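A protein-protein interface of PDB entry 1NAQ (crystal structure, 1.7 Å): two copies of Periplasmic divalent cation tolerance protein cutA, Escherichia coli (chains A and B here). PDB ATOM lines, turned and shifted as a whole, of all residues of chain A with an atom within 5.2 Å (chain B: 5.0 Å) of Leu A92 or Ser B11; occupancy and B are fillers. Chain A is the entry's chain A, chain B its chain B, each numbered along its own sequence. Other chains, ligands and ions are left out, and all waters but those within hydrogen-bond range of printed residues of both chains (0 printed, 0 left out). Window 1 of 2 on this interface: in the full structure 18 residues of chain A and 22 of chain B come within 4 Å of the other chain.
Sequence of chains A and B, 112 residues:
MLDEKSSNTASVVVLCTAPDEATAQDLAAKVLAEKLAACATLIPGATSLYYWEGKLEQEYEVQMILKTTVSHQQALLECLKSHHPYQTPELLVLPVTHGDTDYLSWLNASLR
The side-chain amino group (NZ) of Lys B67 is in salt-bridge range of the side-chain carboxylate (OE2) of Glu A90, at 3.0 Å.
OE2 of Glu A90 sits at hydrogen-bond distance from OH of Tyr B103.
The backbone NH (N) of Val A93 is in hydrogen-bond range of the backbone carbonyl oxygen (O) of His B98 (2.9 Å).
Among the printed residues, pairs that only touch across the chains: Leu A91 with Gly B99 (3.2 Å), Leu A92 with Ser B11 (3.96 Å), Leu A92 with Lys B67 (3.9 Å), Leu A92 with His B98 (3.7 Å), Val A93 with Val B96 (3.4 Å), Leu A94 with Pro B95 (3.5 Å) and Leu A94 with Val B96 (3.9 Å).
The backbone carbonyl oxygen (O) of Val A13 is in hydrogen-bond range of the backbone NH (N) of Leu A94, at 2.7 Å.
The backbone NH of Leu A15 sits at hydrogen-bond distance from the backbone carbonyl oxygen of Leu A92, 2.8 Å away.
Printed residues of chain B within 4 Å of Leu A91: Gly B99 (3.2 Å).
Printed residues of chain B within 4 Å of Leu A92: Ser B11, Lys B67 and His B98.
Printed residues of chain A within 4 Å of Ser B11: Leu A92 (3.96 Å).
Printed residues of chain A within 4 Å of Lys B67: Glu A90 and Leu A92.
Val B70 touches none of the printed residues of chain A.
Printed residues of chain A within 4 Å of Pro B95: Leu A94.
Of the printed residues of chain A, Gly B99 touches Leu A91.
The nearest printed residue of chain B that does not touch Leu A92 is Val B13 (4.01 Å).
The nearest printed residue of chain B that does not touch Glu A90 is Leu B107 (6.1 Å).
Of the 8 printed residues of chain A, 5 touch a printed residue of chain B.
Printed residues of chain A that touch a printed residue of chain B: Glu A90, Leu A91, Leu A92, Val A93 and Leu A94.
Hydrophobic or aromatic side chains of chain A that line the printed part of chain B: Leu A92, Val A93 and Leu A94.
Of the 16 printed residues of chain B, 7 touch a printed residue of chain A.
1 position is printed for both chains.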
ATOM      1  N   VAL A  13     -14.877   6.851  17.706  1.00  0.00           N
ATOM      2  CA  VAL A  13     -14.589   6.067  18.900  1.00  0.00           C
ATOM      3  C   VAL A  13     -13.941   6.896  19.928  1.00  0.00           C
ATOM      4  O   VAL A  13     -12.989   7.666  19.643  1.00  0.00           O
ATOM      5  CB  VAL A  13     -14.103   4.560  18.776  1.00  0.00           C
ATOM      6  CG1 VAL A  13     -14.428   3.921  17.483  1.00  0.00           C
ATOM      7  CG2 VAL A  13     -12.748   4.256  19.298  1.00  0.00           C
ATOM      8  N   VAL A  14     -14.629   6.900  21.083  1.00  0.00           N
ATOM      9  CA  VAL A  14     -14.111   7.549  22.255  1.00  0.00           C
ATOM     10  C   VAL A  14     -13.583   6.555  23.286  1.00  0.00           C
ATOM     11  O   VAL A  14     -14.264   5.661  23.727  1.00  0.00           O
ATOM     12  CB  VAL A  14     -15.148   8.517  22.860  1.00  0.00           C
ATOM     13  CG1 VAL A  14     -14.432   9.222  23.965  1.00  0.00           C
ATOM     14  CG2 VAL A  14     -15.704   9.467  21.758  1.00  0.00           C
ATOM     15  N   LEU A  15     -12.298   6.683  23.590  1.00  0.00           N
ATOM     16  CA  LEU A  15     -11.602   5.864  24.608  1.00  0.00           C
ATOM     17  C   LEU A  15     -11.604   6.579  25.934  1.00  0.00           C
ATOM     18  O   LEU A  15     -11.173   7.727  26.050  1.00  0.00           O
ATOM     19  CB  LEU A  15     -10.155   5.577  24.197  1.00  0.00           C
ATOM     20  CG  LEU A  15      -9.865   4.829  22.869  1.00  0.00           C
ATOM     21  CD1 LEU A  15      -8.279   4.644  22.671  1.00  0.00           C
ATOM     22  CD2 LEU A  15     -10.706   3.563  22.707  1.00  0.00           C
ATOM     23  N   GLU A  90      -8.819  10.050  31.309  1.00  0.00           N
ATOM     24  CA  GLU A  90      -7.874   9.694  30.251  1.00  0.00           C
ATOM     25  C   GLU A  90      -8.739   9.491  29.026  1.00  0.00           C
ATOM     26  O   GLU A  90      -9.270   8.414  28.845  1.00  0.00           O
ATOM     27  CB  GLU A  90      -7.080   8.377  30.607  1.00  0.00           C
ATOM     28  CG  GLU A  90      -6.238   7.902  29.425  1.00  0.00           C
ATOM     29  CD  GLU A  90      -5.275   6.753  29.740  1.00  0.00           C
ATOM     30  OE1 GLU A  90      -5.729   5.703  30.207  1.00  0.00           O
ATOM     31  OE2 GLU A  90      -4.065   6.896  29.488  1.00  0.00           O
ATOM     32  N   LEU A  91      -8.913  10.511  28.196  1.00  0.00           N
ATOM     33  CA  LEU A  91      -9.976  10.474  27.195  1.00  0.00           C
ATOM     34  C   LEU A  91      -9.503  10.920  25.837  1.00  0.00           C
ATOM     35  O   LEU A  91      -9.047  12.050  25.682  1.00  0.00           O
ATOM     36  CB  LEU A  91     -11.111  11.386  27.640  1.00  0.00           C
ATOM     37  CG  LEU A  91     -12.453  11.533  26.970  1.00  0.00           C
ATOM     38  CD1 LEU A  91     -13.227  12.581  27.851  1.00  0.00           C
ATOM     39  CD2 LEU A  91     -12.506  11.890  25.462  1.00  0.00           C
ATOM     40  N   LEU A  92      -9.638  10.034  24.847  1.00  0.00           N
ATOM     41  CA  LEU A  92      -9.084  10.263  23.520  1.00  0.00           C
ATOM     42  C   LEU A  92     -10.116   9.874  22.467  1.00  0.00           C
ATOM     43  O   LEU A  92     -10.867   8.948  22.654  1.00  0.00           O
ATOM     44  CB  LEU A  92      -7.828   9.395  23.259  1.00  0.00           C
ATOM     45  CG  LEU A  92      -6.750   9.474  24.321  1.00  0.00           C
ATOM     46  CD1 LEU A  92      -5.739   8.270  24.229  1.00  0.00           C
ATOM     47  CD2 LEU A  92      -6.030  10.762  23.964  1.00  0.00           C
ATOM     48  N   VAL A  93     -10.120  10.591  21.374  1.00  0.00           N
ATOM     49  CA  VAL A  93     -11.118  10.384  20.298  1.00  0.00           C
ATOM     50  C   VAL A  93     -10.378   9.900  19.040  1.00  0.00           C
ATOM     51  O   VAL A  93      -9.344  10.482  18.576  1.00  0.00           O
ATOM     52  CB  VAL A  93     -11.821  11.673  19.977  1.00  0.00           C
ATOM     53  CG1 VAL A  93     -12.822  11.498  18.770  1.00  0.00           C
ATOM     54  CG2 VAL A  93     -12.603  12.210  21.259  1.00  0.00           C
ATOM     55  N   LEU A  94     -10.905   8.837  18.459  1.00  0.00           N
ATOM     56  CA  LEU A  94     -10.291   8.305  17.242  1.00  0.00           C
ATOM     57  C   LEU A  94     -11.280   8.402  16.107  1.00  0.00           C
ATOM     58  O   LEU A  94     -12.446   7.998  16.245  1.00  0.00           O
ATOM     59  CB  LEU A  94      -9.903   6.840  17.430  1.00  0.00           C
ATOM     60  CG  LEU A  94      -8.979   6.318  18.551  1.00  0.00           C
ATOM     61  CD1 LEU A  94      -8.569   4.885  18.245  1.00  0.00           C
ATOM     62  CD2 LEU A  94      -7.753   7.168  18.631  1.00  0.00           C
ATOM     63  N   THR B   9       0.098  20.583  21.001  1.00  0.00           N
ATOM     64  CA  THR B   9       0.655  19.191  21.072  1.00  0.00           C
ATOM     65  C   THR B   9      -0.396  18.170  20.615  1.00  0.00           C
ATOM     66  O   THR B   9      -1.457  18.081  21.217  1.00  0.00           O
ATOM     67  CB  THR B   9       1.128  18.885  22.514  1.00  0.00           C
ATOM     68  OG1 THR B   9       2.530  19.146  22.608  1.00  0.00           O
ATOM     69  CG2 THR B   9       1.050  17.384  22.853  1.00  0.00           C
ATOM     70  N   ALA B  10      -0.146  17.456  19.525  1.00  0.00           N
ATOM     71  CA  ALA B  10      -1.051  16.398  19.123  1.00  0.00           C
ATOM     72  C   ALA B  10      -0.583  15.066  19.713  1.00  0.00           C
ATOM     73  O   ALA B  10       0.597  14.815  19.903  1.00  0.00           O
ATOM     74  CB  ALA B  10      -1.157  16.317  17.646  1.00  0.00           C
ATOM     75  N   SER B  11      -1.535  14.217  20.023  1.00  0.00           N
ATOM     76  CA  SER B  11      -1.200  12.901  20.515  1.00  0.00           C
ATOM     77  C   SER B  11      -1.469  11.798  19.481  1.00  0.00           C
ATOM     78  O   SER B  11      -2.180  11.998  18.492  1.00  0.00           O
ATOM     79  CB  SER B  11      -1.939  12.637  21.818  1.00  0.00           C
ATOM     80  OG  SER B  11      -3.294  12.333  21.572  1.00  0.00           O
ATOM     81  N   VAL B  12      -0.873  10.618  19.729  1.00  0.00           N
ATOM     82  CA  VAL B  12      -1.160   9.390  18.965  1.00  0.00           C
ATOM     83  C   VAL B  12      -1.285   8.172  19.892  1.00  0.00           C
ATOM     84  O   VAL B  12      -0.797   8.191  21.008  1.00  0.00           O
ATOM     85  CB  VAL B  12      -0.114   9.079  17.872  1.00  0.00           C
ATOM     86  CG1 VAL B  12      -0.095  10.190  16.789  1.00  0.00           C
ATOM     87  CG2 VAL B  12       1.280   8.799  18.460  1.00  0.00           C
ATOM     88  N   VAL B  13      -1.986   7.149  19.409  1.00  0.00           N
ATOM     89  CA  VAL B  13      -2.029   5.834  20.025  1.00  0.00           C
ATOM     90  C   VAL B  13      -1.175   4.882  19.199  1.00  0.00           C
ATOM     91  O   VAL B  13      -1.321   4.762  17.975  1.00  0.00           O
ATOM     92  CB  VAL B  13      -3.514   5.361  20.095  1.00  0.00           C
ATOM     93  CG1 VAL B  13      -3.656   3.843  20.450  1.00  0.00           C
ATOM     94  CG2 VAL B  13      -4.258   6.273  21.082  1.00  0.00           C
ATOM     95  N   LYS B  67       0.494   5.588  24.630  1.00  0.00           N
ATOM     96  CA  LYS B  67       0.124   6.949  24.336  1.00  0.00           C
ATOM     97  C   LYS B  67       1.275   7.935  24.426  1.00  0.00           C
ATOM     98  O   LYS B  67       2.009   8.010  25.427  1.00  0.00           O
ATOM     99  CB  LYS B  67      -1.022   7.378  25.264  1.00  0.00           C
ATOM    100  CG  LYS B  67      -2.310   6.475  24.922  1.00  0.00           C
ATOM    101  CD  LYS B  67      -3.076   6.132  26.179  1.00  0.00           C
ATOM    102  CE  LYS B  67      -2.571   4.853  26.891  1.00  0.00           C
ATOM    103  NZ  LYS B  67      -3.640   4.414  27.890  1.00  0.00           N
ATOM    104  N   THR B  68       1.452   8.685  23.355  1.00  0.00           N
ATOM    105  CA  THR B  68       2.644   9.527  23.178  1.00  0.00           C
ATOM    106  C   THR B  68       2.271  10.755  22.329  1.00  0.00           C
ATOM    107  O   THR B  68       1.038  10.985  22.073  1.00  0.00           O
ATOM    108  CB  THR B  68       3.904   8.754  22.663  1.00  0.00           C
ATOM    109  OG1 THR B  68       5.023   9.631  22.821  1.00  0.00           O
ATOM    110  CG2 THR B  68       3.847   8.447  21.193  1.00  0.00           C
ATOM    111  N   THR B  69       3.221  11.655  22.056  1.00  0.00           N
ATOM    112  CA  THR B  69       2.923  12.803  21.150  1.00  0.00           C
ATOM    113  C   THR B  69       3.563  12.622  19.782  1.00  0.00           C
ATOM    114  O   THR B  69       4.469  11.805  19.616  1.00  0.00           O
ATOM    115  CB  THR B  69       3.362  14.141  21.723  1.00  0.00           C
ATOM    116  OG1 THR B  69       4.781  14.135  21.936  1.00  0.00           O
ATOM    117  CG2 THR B  69       2.742  14.414  23.099  1.00  0.00           C
ATOM    118  N   VAL B  70       3.071  13.326  18.771  1.00  0.00           N
ATOM    119  CA  VAL B  70       3.654  13.147  17.438  1.00  0.00           C
ATOM    120  C   VAL B  70       5.165  13.385  17.396  1.00  0.00           C
ATOM    121  O   VAL B  70       5.903  12.772  16.584  1.00  0.00           O
ATOM    122  CB  VAL B  70       2.983  14.102  16.436  1.00  0.00           C
ATOM    123  CG1 VAL B  70       1.604  13.597  16.167  1.00  0.00           C
ATOM    124  CG2 VAL B  70       2.941  15.521  17.005  1.00  0.00           C
ATOM    125  N   PRO B  95      -4.181   7.822  14.474  1.00  0.00           N
ATOM    126  CA  PRO B  95      -4.304   9.244  14.810  1.00  0.00           C
ATOM    127  C   PRO B  95      -5.397   9.518  15.840  1.00  0.00           C
ATOM    128  O   PRO B  95      -6.455   8.855  15.826  1.00  0.00           O
ATOM    129  CB  PRO B  95      -4.764   9.883  13.495  1.00  0.00           C
ATOM    130  CG  PRO B  95      -5.568   8.826  12.836  1.00  0.00           C
ATOM    131  CD  PRO B  95      -4.774   7.538  13.153  1.00  0.00           C
ATOM    132  N   VAL B  96      -5.124  10.493  16.688  1.00  0.00           N
ATOM    133  CA  VAL B  96      -6.084  11.016  17.673  1.00  0.00           C
ATOM    134  C   VAL B  96      -6.538  12.375  17.220  1.00  0.00           C
ATOM    135  O   VAL B  96      -5.733  13.255  16.998  1.00  0.00           O
ATOM    136  CB  VAL B  96      -5.414  11.133  19.063  1.00  0.00           C
ATOM    137  CG1 VAL B  96      -6.344  11.867  20.074  1.00  0.00           C
ATOM    138  CG2 VAL B  96      -4.991   9.729  19.575  1.00  0.00           C
ATOM    139  N   HIS B  98      -8.988  14.243  18.955  1.00  0.00           N
ATOM    140  CA  HIS B  98      -9.297  15.157  20.083  1.00  0.00           C
ATOM    141  C   HIS B  98      -9.291  14.432  21.381  1.00  0.00           C
ATOM    142  O   HIS B  98      -9.027  13.273  21.441  1.00  0.00           O
ATOM    143  CB  HIS B  98     -10.660  15.789  19.885  1.00  0.00           C
ATOM    144  CG  HIS B  98     -10.891  17.041  20.689  1.00  0.00           C
ATOM    145  ND1 HIS B  98     -10.145  18.194  20.533  1.00  0.00           N
ATOM    146  CD2 HIS B  98     -11.872  17.351  21.568  1.00  0.00           C
ATOM    147  CE1 HIS B  98     -10.637  19.145  21.312  1.00  0.00           C
ATOM    148  NE2 HIS B  98     -11.681  18.656  21.959  1.00  0.00           N
ATOM    149  N   GLY B  99      -9.665  15.119  22.447  1.00  0.00           N
ATOM    150  CA  GLY B  99      -9.765  14.449  23.741  1.00  0.00           C
ATOM    151  C   GLY B  99      -9.917  15.451  24.877  1.00  0.00           C
ATOM    152  O   GLY B  99     -10.313  16.625  24.695  1.00  0.00           O
ATOM    153  N   TYR B 103      -5.844  16.208  30.099  1.00  0.00           N
ATOM    154  CA  TYR B 103      -5.070  14.972  29.879  1.00  0.00           C
ATOM    155  C   TYR B 103      -3.990  15.194  28.848  1.00  0.00           C
ATOM    156  O   TYR B 103      -2.852  14.693  28.997  1.00  0.00           O
ATOM    157  CB  TYR B 103      -5.976  13.820  29.476  1.00  0.00           C
ATOM    158  CG  TYR B 103      -5.184  12.548  29.244  1.00  0.00           C
ATOM    159  CD1 TYR B 103      -4.939  12.087  27.972  1.00  0.00           C
ATOM    160  CD2 TYR B 103      -4.653  11.840  30.318  1.00  0.00           C
ATOM    161  CE1 TYR B 103      -4.174  10.898  27.763  1.00  0.00           C
ATOM    162  CE2 TYR B 103      -3.884  10.633  30.129  1.00  0.00           C
ATOM    163  CZ  TYR B 103      -3.650  10.178  28.854  1.00  0.00           C
ATOM    164  OH  TYR B 103      -2.904   9.018  28.561  1.00  0.00           O
ATOM    165  N   LEU B 104      -4.339  15.867  27.748  1.00  0.00           N
ATOM    166  CA  LEU B 104      -3.358  16.105  26.731  1.00  0.00           C
ATOM    167  C   LEU B 104      -2.192  16.988  27.157  1.00  0.00           C
ATOM    168  O   LEU B 104      -1.051  16.728  26.795  1.00  0.00           O
ATOM    169  CB  LEU B 104      -4.001  16.586  25.420  1.00  0.00           C
ATOM    170  CG  LEU B 104      -3.609  15.504  24.390  1.00  0.00           C
ATOM    171  CD1 LEU B 104      -4.806  14.629  24.024  1.00  0.00           C
ATOM    172  CD2 LEU B 104      -2.849  16.044  23.142  1.00  0.00           C
ATOM    173  N   LEU B 107       0.120  14.710  28.873  1.00  0.00           N
ATOM    174  CA  LEU B 107       0.915  13.928  27.917  1.00  0.00           C
ATOM    175  C   LEU B 107       2.135  14.688  27.497  1.00  0.00           C
ATOM    176  O   LEU B 107       3.240  14.126  27.393  1.00  0.00           O
ATOM    177  CB  LEU B 107       0.136  13.651  26.639  1.00  0.00           C
ATOM    178  CG  LEU B 107      -0.753  12.420  26.608  1.00  0.00           C
ATOM    179  CD1 LEU B 107      -0.977  12.058  25.154  1.00  0.00           C
ATOM    180  CD2 LEU B 107      -0.277  11.209  27.377  1.00  0.00           C
